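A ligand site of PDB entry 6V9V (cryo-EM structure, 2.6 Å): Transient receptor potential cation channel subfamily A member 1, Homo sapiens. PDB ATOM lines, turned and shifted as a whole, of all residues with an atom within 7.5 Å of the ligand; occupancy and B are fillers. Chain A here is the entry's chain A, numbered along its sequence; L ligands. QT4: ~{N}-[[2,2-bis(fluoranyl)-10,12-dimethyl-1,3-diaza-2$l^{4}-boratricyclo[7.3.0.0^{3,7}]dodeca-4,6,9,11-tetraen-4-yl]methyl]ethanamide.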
ATOM      1  N   ASP A 606       2.759  -4.325 -12.762  1.00  0.00           N
ATOM      2  CA  ASP A 606       2.307  -2.949 -12.929  1.00  0.00           C
ATOM      3  C   ASP A 606       3.417  -2.054 -13.439  1.00  0.00           C
ATOM      4  O   ASP A 606       3.166  -1.140 -14.227  1.00  0.00           O
ATOM      5  CB  ASP A 606       1.771  -2.428 -11.606  1.00  0.00           C
ATOM      6  CG  ASP A 606       0.457  -3.075 -11.228  1.00  0.00           C
ATOM      7  OD1 ASP A 606      -0.155  -3.696 -12.112  1.00  0.00           O
ATOM      8  OD2 ASP A 606       0.046  -2.958 -10.060  1.00  0.00           O
ATOM      9  N   LEU A 609       3.709  -2.454 -16.913  1.00  0.00           N
ATOM     10  CA  LEU A 609       2.508  -1.986 -17.585  1.00  0.00           C
ATOM     11  C   LEU A 609       2.614  -0.499 -17.896  1.00  0.00           C
ATOM     12  O   LEU A 609       2.236  -0.060 -18.983  1.00  0.00           O
ATOM     13  CB  LEU A 609       1.283  -2.261 -16.731  1.00  0.00           C
ATOM     14  CG  LEU A 609      -0.027  -1.998 -17.455  1.00  0.00           C
ATOM     15  CD1 LEU A 609      -0.285  -3.110 -18.441  1.00  0.00           C
ATOM     16  CD2 LEU A 609      -1.177  -1.867 -16.474  1.00  0.00           C
ATOM     17  N   LYS A 610       3.136   0.278 -16.954  1.00  0.00           N
ATOM     18  CA  LYS A 610       3.261   1.720 -17.111  1.00  0.00           C
ATOM     19  C   LYS A 610       4.570   2.128 -17.745  1.00  0.00           C
ATOM     20  O   LYS A 610       4.872   3.326 -17.796  1.00  0.00           O
ATOM     21  CB  LYS A 610       3.102   2.404 -15.755  1.00  0.00           C
ATOM     22  CG  LYS A 610       4.182   2.016 -14.776  1.00  0.00           C
ATOM     23  CD  LYS A 610       3.819   2.464 -13.369  1.00  0.00           C
ATOM     24  CE  LYS A 610       4.968   2.217 -12.407  1.00  0.00           C
ATOM     25  NZ  LYS A 610       4.606   2.618 -11.023  1.00  0.00           N
ATOM     26  N   ILE A 611       5.366   1.176 -18.237  1.00  0.00           N
ATOM     27  CA  ILE A 611       6.687   1.491 -18.764  1.00  0.00           C
ATOM     28  C   ILE A 611       6.621   1.890 -20.234  1.00  0.00           C
ATOM     29  O   ILE A 611       7.647   2.327 -20.802  1.00  0.00           O
ATOM     30  CB  ILE A 611       7.608   0.278 -18.538  1.00  0.00           C
ATOM     31  CG1 ILE A 611       9.080   0.708 -18.456  1.00  0.00           C
ATOM     32  CG2 ILE A 611       7.408  -0.751 -19.625  1.00  0.00           C
ATOM     33  CD1 ILE A 611       9.358   1.671 -17.332  1.00  0.00           C
ATOM     34  N   PHE A 612       5.455   1.802 -20.858  1.00  0.00           N
ATOM     35  CA  PHE A 612       5.310   2.167 -22.263  1.00  0.00           C
ATOM     36  C   PHE A 612       5.417   3.675 -22.439  1.00  0.00           C
ATOM     37  O   PHE A 612       5.373   4.456 -21.497  1.00  0.00           O
ATOM     38  CB  PHE A 612       3.965   1.682 -22.795  1.00  0.00           C
ATOM     39  CG  PHE A 612       2.810   2.547 -22.418  1.00  0.00           C
ATOM     40  CD1 PHE A 612       2.332   2.572 -21.121  1.00  0.00           C
ATOM     41  CD2 PHE A 612       2.175   3.332 -23.370  1.00  0.00           C
ATOM     42  CE1 PHE A 612       1.264   3.359 -20.771  1.00  0.00           C
ATOM     43  CE2 PHE A 612       1.100   4.124 -23.031  1.00  0.00           C
ATOM     44  CZ  PHE A 612       0.651   4.141 -21.729  1.00  0.00           C
ATOM     45  N   HIS A 614       4.055   7.086 -24.909  1.00  0.00           N
ATOM     46  CA  HIS A 614       3.063   7.615 -25.827  1.00  0.00           C
ATOM     47  C   HIS A 614       3.762   8.096 -27.089  1.00  0.00           C
ATOM     48  O   HIS A 614       4.956   7.857 -27.292  1.00  0.00           O
ATOM     49  CB  HIS A 614       2.253   8.731 -25.167  1.00  0.00           C
ATOM     50  CG  HIS A 614       1.877   8.451 -23.750  1.00  0.00           C
ATOM     51  ND1 HIS A 614       0.662   7.896 -23.395  1.00  0.00           N
ATOM     52  CD2 HIS A 614       2.542   8.651 -22.585  1.00  0.00           C
ATOM     53  CE1 HIS A 614       0.605   7.775 -22.081  1.00  0.00           C
ATOM     54  NE2 HIS A 614       1.736   8.214 -21.568  1.00  0.00           N
ATOM     55  N   LYS A 620       1.957   0.838 -28.533  1.00  0.00           N
ATOM     56  CA  LYS A 620       1.083   1.739 -27.797  1.00  0.00           C
ATOM     57  C   LYS A 620       0.981   1.341 -26.332  1.00  0.00           C
ATOM     58  O   LYS A 620       1.960   0.915 -25.713  1.00  0.00           O
ATOM     59  CB  LYS A 620      -0.303   1.761 -28.423  1.00  0.00           C
ATOM     60  CG  LYS A 620      -0.267   1.759 -29.936  1.00  0.00           C
ATOM     61  CD  LYS A 620      -1.638   1.441 -30.497  1.00  0.00           C
ATOM     62  CE  LYS A 620      -1.597   1.383 -32.012  1.00  0.00           C
ATOM     63  NZ  LYS A 620      -2.922   0.984 -32.559  1.00  0.00           N
ATOM     64  N   CYS A 621      -0.209   1.489 -25.765  1.00  0.00           N
ATOM     65  CA  CYS A 621      -0.453   1.087 -24.407  1.00  0.00           C
ATOM     66  C   CYS A 621      -0.547  -0.429 -24.411  1.00  0.00           C
ATOM     67  O   CYS A 621      -1.282  -0.984 -25.269  1.00  0.00           O
ATOM     68  CB  CYS A 621      -1.745   1.750 -23.938  1.00  0.00           C
ATOM     69  SG  CYS A 621      -2.623   0.626 -22.821  1.00  0.00           S
ATOM     70  N   PRO A 622       0.151  -1.102 -23.486  1.00  0.00           N
ATOM     71  CA  PRO A 622       0.313  -2.564 -23.456  1.00  0.00           C
ATOM     72  C   PRO A 622      -0.980  -3.341 -23.385  1.00  0.00           C
ATOM     73  O   PRO A 622      -1.043  -4.482 -23.851  1.00  0.00           O
ATOM     74  CB  PRO A 622       1.129  -2.795 -22.190  1.00  0.00           C
ATOM     75  CG  PRO A 622       1.812  -1.523 -21.941  1.00  0.00           C
ATOM     76  CD  PRO A 622       0.843  -0.475 -22.353  1.00  0.00           C
ATOM     77  N   ILE A 623      -2.006  -2.733 -22.791  1.00  0.00           N
ATOM     78  CA  ILE A 623      -3.329  -3.341 -22.781  1.00  0.00           C
ATOM     79  C   ILE A 623      -3.884  -3.414 -24.181  1.00  0.00           C
ATOM     80  O   ILE A 623      -4.453  -4.434 -24.588  1.00  0.00           O
ATOM     81  CB  ILE A 623      -4.252  -2.563 -21.834  1.00  0.00           C
ATOM     82  CG1 ILE A 623      -3.713  -2.624 -20.409  1.00  0.00           C
ATOM     83  CG2 ILE A 623      -5.655  -3.115 -21.864  1.00  0.00           C
ATOM     84  CD1 ILE A 623      -3.689  -4.014 -19.842  1.00  0.00           C
ATOM     85  N   THR A 624      -3.681  -2.355 -24.973  1.00  0.00           N
ATOM     86  CA  THR A 624      -4.279  -2.288 -26.306  1.00  0.00           C
ATOM     87  C   THR A 624      -3.653  -3.299 -27.269  1.00  0.00           C
ATOM     88  O   THR A 624      -4.352  -3.842 -28.126  1.00  0.00           O
ATOM     89  CB  THR A 624      -4.159  -0.882 -26.870  1.00  0.00           C
ATOM     90  OG1 THR A 624      -4.861   0.030 -26.007  1.00  0.00           O
ATOM     91  CG2 THR A 624      -4.756  -0.809 -28.254  1.00  0.00           C
ATOM     92  N   LYS A 661      -9.423  -1.750 -13.021  1.00  0.00           N
ATOM     93  CA  LYS A 661      -8.203  -0.966 -13.089  1.00  0.00           C
ATOM     94  C   LYS A 661      -7.529  -1.046 -14.440  1.00  0.00           C
ATOM     95  O   LYS A 661      -6.735  -0.161 -14.776  1.00  0.00           O
ATOM     96  CB  LYS A 661      -7.226  -1.406 -12.003  1.00  0.00           C
ATOM     97  CG  LYS A 661      -6.977  -2.900 -11.978  1.00  0.00           C
ATOM     98  CD  LYS A 661      -5.827  -3.234 -11.050  1.00  0.00           C
ATOM     99  CE  LYS A 661      -5.794  -4.724 -10.743  1.00  0.00           C
ATOM    100  NZ  LYS A 661      -4.675  -5.058  -9.824  1.00  0.00           N
ATOM    101  N   TYR A 662      -7.820  -2.074 -15.231  1.00  0.00           N
ATOM    102  CA  TYR A 662      -7.166  -2.270 -16.511  1.00  0.00           C
ATOM    103  C   TYR A 662      -8.041  -1.869 -17.686  1.00  0.00           C
ATOM    104  O   TYR A 662      -7.590  -1.949 -18.832  1.00  0.00           O
ATOM    105  CB  TYR A 662      -6.738  -3.726 -16.672  1.00  0.00           C
ATOM    106  CG  TYR A 662      -5.705  -4.142 -15.670  1.00  0.00           C
ATOM    107  CD1 TYR A 662      -4.651  -3.296 -15.341  1.00  0.00           C
ATOM    108  CD2 TYR A 662      -5.770  -5.375 -15.045  1.00  0.00           C
ATOM    109  CE1 TYR A 662      -3.702  -3.661 -14.425  1.00  0.00           C
ATOM    110  CE2 TYR A 662      -4.817  -5.756 -14.121  1.00  0.00           C
ATOM    111  CZ  TYR A 662      -3.786  -4.896 -13.817  1.00  0.00           C
ATOM    112  OH  TYR A 662      -2.839  -5.271 -12.904  1.00  0.00           O
ATOM    113  N   LEU A 663      -9.270  -1.450 -17.445  1.00  0.00           N
ATOM    114  CA  LEU A 663     -10.196  -1.185 -18.531  1.00  0.00           C
ATOM    115  C   LEU A 663     -10.260   0.287 -18.927  1.00  0.00           C
ATOM    116  O   LEU A 663     -11.050   0.635 -19.813  1.00  0.00           O
ATOM    117  CB  LEU A 663     -11.593  -1.658 -18.153  1.00  0.00           C
ATOM    118  CG  LEU A 663     -11.698  -3.153 -17.855  1.00  0.00           C
ATOM    119  CD1 LEU A 663     -13.109  -3.532 -17.520  1.00  0.00           C
ATOM    120  CD2 LEU A 663     -11.214  -3.945 -19.038  1.00  0.00           C
ATOM    121  N   GLN A 664      -9.453   1.144 -18.312  1.00  0.00           N
ATOM    122  CA  GLN A 664      -9.700   2.570 -18.460  1.00  0.00           C
ATOM    123  C   GLN A 664      -8.450   3.376 -18.161  1.00  0.00           C
ATOM    124  O   GLN A 664      -7.599   2.959 -17.373  1.00  0.00           O
ATOM    125  CB  GLN A 664     -10.829   3.003 -17.523  1.00  0.00           C
ATOM    126  CG  GLN A 664     -11.625   4.188 -17.989  1.00  0.00           C
ATOM    127  CD  GLN A 664     -12.600   4.640 -16.938  1.00  0.00           C
ATOM    128  OE1 GLN A 664     -12.403   4.407 -15.741  1.00  0.00           O
ATOM    129  NE2 GLN A 664     -13.657   5.305 -17.367  1.00  0.00           N
ATOM    130  N   CYS A 665      -8.361   4.542 -18.797  1.00  0.00           N
ATOM    131  CA  CYS A 665      -7.455   5.589 -18.372  1.00  0.00           C
ATOM    132  C   CYS A 665      -7.980   6.225 -17.080  1.00  0.00           C
ATOM    133  O   CYS A 665      -9.137   6.020 -16.714  1.00  0.00           O
ATOM    134  CB  CYS A 665      -7.299   6.642 -19.468  1.00  0.00           C
ATOM    135  SG  CYS A 665      -6.632   6.029 -21.003  1.00  0.00           S
ATOM    136  N   PRO A 666      -7.161   7.032 -16.389  1.00  0.00           N
ATOM    137  CA  PRO A 666      -7.692   7.793 -15.238  1.00  0.00           C
ATOM    138  C   PRO A 666      -8.544   9.016 -15.580  1.00  0.00           C
ATOM    139  O   PRO A 666      -8.699   9.890 -14.732  1.00  0.00           O
ATOM    140  CB  PRO A 666      -6.425   8.205 -14.489  1.00  0.00           C
ATOM    141  CG  PRO A 666      -5.425   7.194 -14.864  1.00  0.00           C
ATOM    142  CD  PRO A 666      -5.699   6.883 -16.288  1.00  0.00           C
ATOM    143  N   LEU A 667      -9.009   9.110 -16.836  1.00  0.00           N
ATOM    144  CA  LEU A 667      -9.994  10.064 -17.373  1.00  0.00           C
ATOM    145  C   LEU A 667      -9.450  11.469 -17.548  1.00  0.00           C
ATOM    146  O   LEU A 667     -10.128  12.323 -18.120  1.00  0.00           O
ATOM    147  CB  LEU A 667     -11.265  10.106 -16.524  1.00  0.00           C
ATOM    148  CG  LEU A 667     -12.028   8.795 -16.334  1.00  0.00           C
ATOM    149  CD1 LEU A 667     -12.471   8.654 -14.889  1.00  0.00           C
ATOM    150  CD2 LEU A 667     -13.224   8.752 -17.266  1.00  0.00           C
ATOM    151  N   GLU A 668      -8.235  11.741 -17.087  1.00  0.00           N
ATOM    152  CA  GLU A 668      -7.617  13.022 -17.402  1.00  0.00           C
ATOM    153  C   GLU A 668      -7.085  13.055 -18.817  1.00  0.00           C
ATOM    154  O   GLU A 668      -6.901  14.137 -19.372  1.00  0.00           O
ATOM    155  CB  GLU A 668      -6.485  13.326 -16.420  1.00  0.00           C
ATOM    156  CG  GLU A 668      -6.940  13.590 -15.012  1.00  0.00           C
ATOM    157  CD  GLU A 668      -6.883  12.354 -14.149  1.00  0.00           C
ATOM    158  OE1 GLU A 668      -5.973  11.529 -14.361  1.00  0.00           O
ATOM    159  OE2 GLU A 668      -7.753  12.204 -13.258  1.00  0.00           O
ATOM    160  N   PHE A 669      -6.849  11.892 -19.417  1.00  0.00           N
ATOM    161  CA  PHE A 669      -6.373  11.790 -20.777  1.00  0.00           C
ATOM    162  C   PHE A 669      -7.498  11.598 -21.771  1.00  0.00           C
ATOM    163  O   PHE A 669      -7.258  11.310 -22.946  1.00  0.00           O
ATOM    164  CB  PHE A 669      -5.375  10.638 -20.889  1.00  0.00           C
ATOM    165  CG  PHE A 669      -4.411  10.561 -19.743  1.00  0.00           C
ATOM    166  CD1 PHE A 669      -3.356  11.456 -19.659  1.00  0.00           C
ATOM    167  CD2 PHE A 669      -4.564   9.616 -18.747  1.00  0.00           C
ATOM    168  CE1 PHE A 669      -2.471  11.408 -18.603  1.00  0.00           C
ATOM    169  CE2 PHE A 669      -3.684   9.556 -17.685  1.00  0.00           C
ATOM    170  CZ  PHE A 669      -2.630  10.444 -17.613  1.00  0.00           C
ATOM    171  N   VAL A 678      -2.143  13.553 -24.008  1.00  0.00           N
ATOM    172  CA  VAL A 678      -2.749  12.292 -24.414  1.00  0.00           C
ATOM    173  C   VAL A 678      -4.232  12.521 -24.703  1.00  0.00           C
ATOM    174  O   VAL A 678      -4.929  13.211 -23.961  1.00  0.00           O
ATOM    175  CB  VAL A 678      -2.552  11.221 -23.339  1.00  0.00           C
ATOM    176  N   TYR A 680      -6.498   9.899 -25.380  1.00  0.00           N
ATOM    177  CA  TYR A 680      -7.096   8.568 -25.352  1.00  0.00           C
ATOM    178  C   TYR A 680      -8.602   8.658 -25.115  1.00  0.00           C
ATOM    179  O   TYR A 680      -9.044   9.078 -24.050  1.00  0.00           O
ATOM    180  CB  TYR A 680      -6.457   7.722 -24.253  1.00  0.00           C
ATOM    181  CG  TYR A 680      -4.989   7.474 -24.445  1.00  0.00           C
ATOM    182  CD1 TYR A 680      -4.455   7.307 -25.719  1.00  0.00           C
ATOM    183  CD2 TYR A 680      -4.129   7.400 -23.361  1.00  0.00           C
ATOM    184  CE1 TYR A 680      -3.103   7.073 -25.898  1.00  0.00           C
ATOM    185  CE2 TYR A 680      -2.790   7.174 -23.519  1.00  0.00           C
ATOM    186  CZ  TYR A 680      -2.279   7.002 -24.791  1.00  0.00           C
ATOM    187  OH  TYR A 680      -0.928   6.775 -24.957  1.00  0.00           O
ATOM    188  N   THR A 684     -11.254   2.560 -22.982  1.00  0.00           N
ATOM    189  CA  THR A 684     -10.168   2.265 -23.907  1.00  0.00           C
ATOM    190  C   THR A 684     -10.074   0.780 -24.213  1.00  0.00           C
ATOM    191  O   THR A 684      -9.899   0.398 -25.378  1.00  0.00           O
ATOM    192  CB  THR A 684      -8.853   2.754 -23.328  1.00  0.00           C
ATOM    193  OG1 THR A 684      -8.593   2.024 -22.125  1.00  0.00           O
ATOM    194  CG2 THR A 684      -8.970   4.182 -23.000  1.00  0.00           C
ATOM    195  N   ALA A 685     -10.178  -0.064 -23.198  1.00  0.00           N
ATOM    196  CA  ALA A 685     -10.068  -1.490 -23.431  1.00  0.00           C
ATOM    197  C   ALA A 685     -11.283  -2.029 -24.166  1.00  0.00           C
ATOM    198  O   ALA A 685     -11.158  -2.939 -24.979  1.00  0.00           O
ATOM    199  CB  ALA A 685      -9.878  -2.230 -22.112  1.00  0.00           C
HETATM  200  C10 QT4 L   1      -2.101   6.073 -18.773  1.00  0.00           C
HETATM  201  B01 QT4 L   1      -2.238   4.451 -16.930  1.00  0.00           B
HETATM  202  C03 QT4 L   1      -0.899   6.490 -16.627  1.00  0.00           C
HETATM  203  C04 QT4 L   1      -0.101   7.112 -15.657  1.00  0.00           C
HETATM  204  C05 QT4 L   1       0.619   8.444 -15.812  1.00  0.00           C
HETATM  205  C06 QT4 L   1      -0.094   6.265 -14.557  1.00  0.00           C
HETATM  206  C07 QT4 L   1      -0.884   5.177 -14.885  1.00  0.00           C
HETATM  207  C08 QT4 L   1      -1.172   3.993 -13.978  1.00  0.00           C
HETATM  208  C09 QT4 L   1      -1.243   6.914 -17.955  1.00  0.00           C
HETATM  209  C12 QT4 L   1      -3.311   4.341 -19.218  1.00  0.00           C
HETATM  210  C13 QT4 L   1      -4.024   3.003 -19.052  1.00  0.00           C
HETATM  211  C15 QT4 L   1      -4.329   2.065 -21.335  1.00  0.00           C
HETATM  212  C17 QT4 L   1      -2.926   1.460 -21.253  1.00  0.00           C
HETATM  213  C25 QT4 L   1      -3.339   5.131 -20.360  1.00  0.00           C
HETATM  214  C26 QT4 L   1      -2.571   6.252 -20.084  1.00  0.00           C
HETATM  215  F27 QT4 L   1      -1.421   3.005 -17.095  1.00  0.00           F
HETATM  216  F28 QT4 L   1      -3.679   4.316 -16.102  1.00  0.00           F
HETATM  217  N02 QT4 L   1      -1.346   5.354 -16.129  1.00  0.00           N
HETATM  218  N11 QT4 L   1      -2.554   4.935 -18.299  1.00  0.00           N
HETATM  219  N14 QT4 L   1      -4.852   2.826 -20.224  1.00  0.00           N
HETATM  220  O16 QT4 L   1      -4.978   1.904 -22.303  1.00  0.00           O
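The side-chain sulfur (SG) of Cys 621 lies close to the backbone NH (N) of Ile 623 (3.4 Å). N of Tyr 680 sits at hydrogen-bond distance from O of Phe 669. A ring nitrogen (ND1) of His 614 sits at hydrogen-bond distance from the side-chain hydroxyl of Tyr 680 (2.5 Å).
SG of Cys 621 is bonded to C17 of the ligand (1.8 Å). The side-chain sulfur (SG) of Cys 665 sits close to a nitrogen (N14) of the ligand.
Residues that only touch the ligand: Gln 664 (3.9 Å), Pro 666 (3.3 Å), Phe 669 (3.6 Å), Tyr 680 (3.6 Å) and Thr 684 (3.6 Å). Hydrophobic or aromatic side chains within 4 Å of the ligand: Pro 666, Phe 669 and Tyr 680. Along chain A the residues within 4 Å of the ligand span positions 621 to 684.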
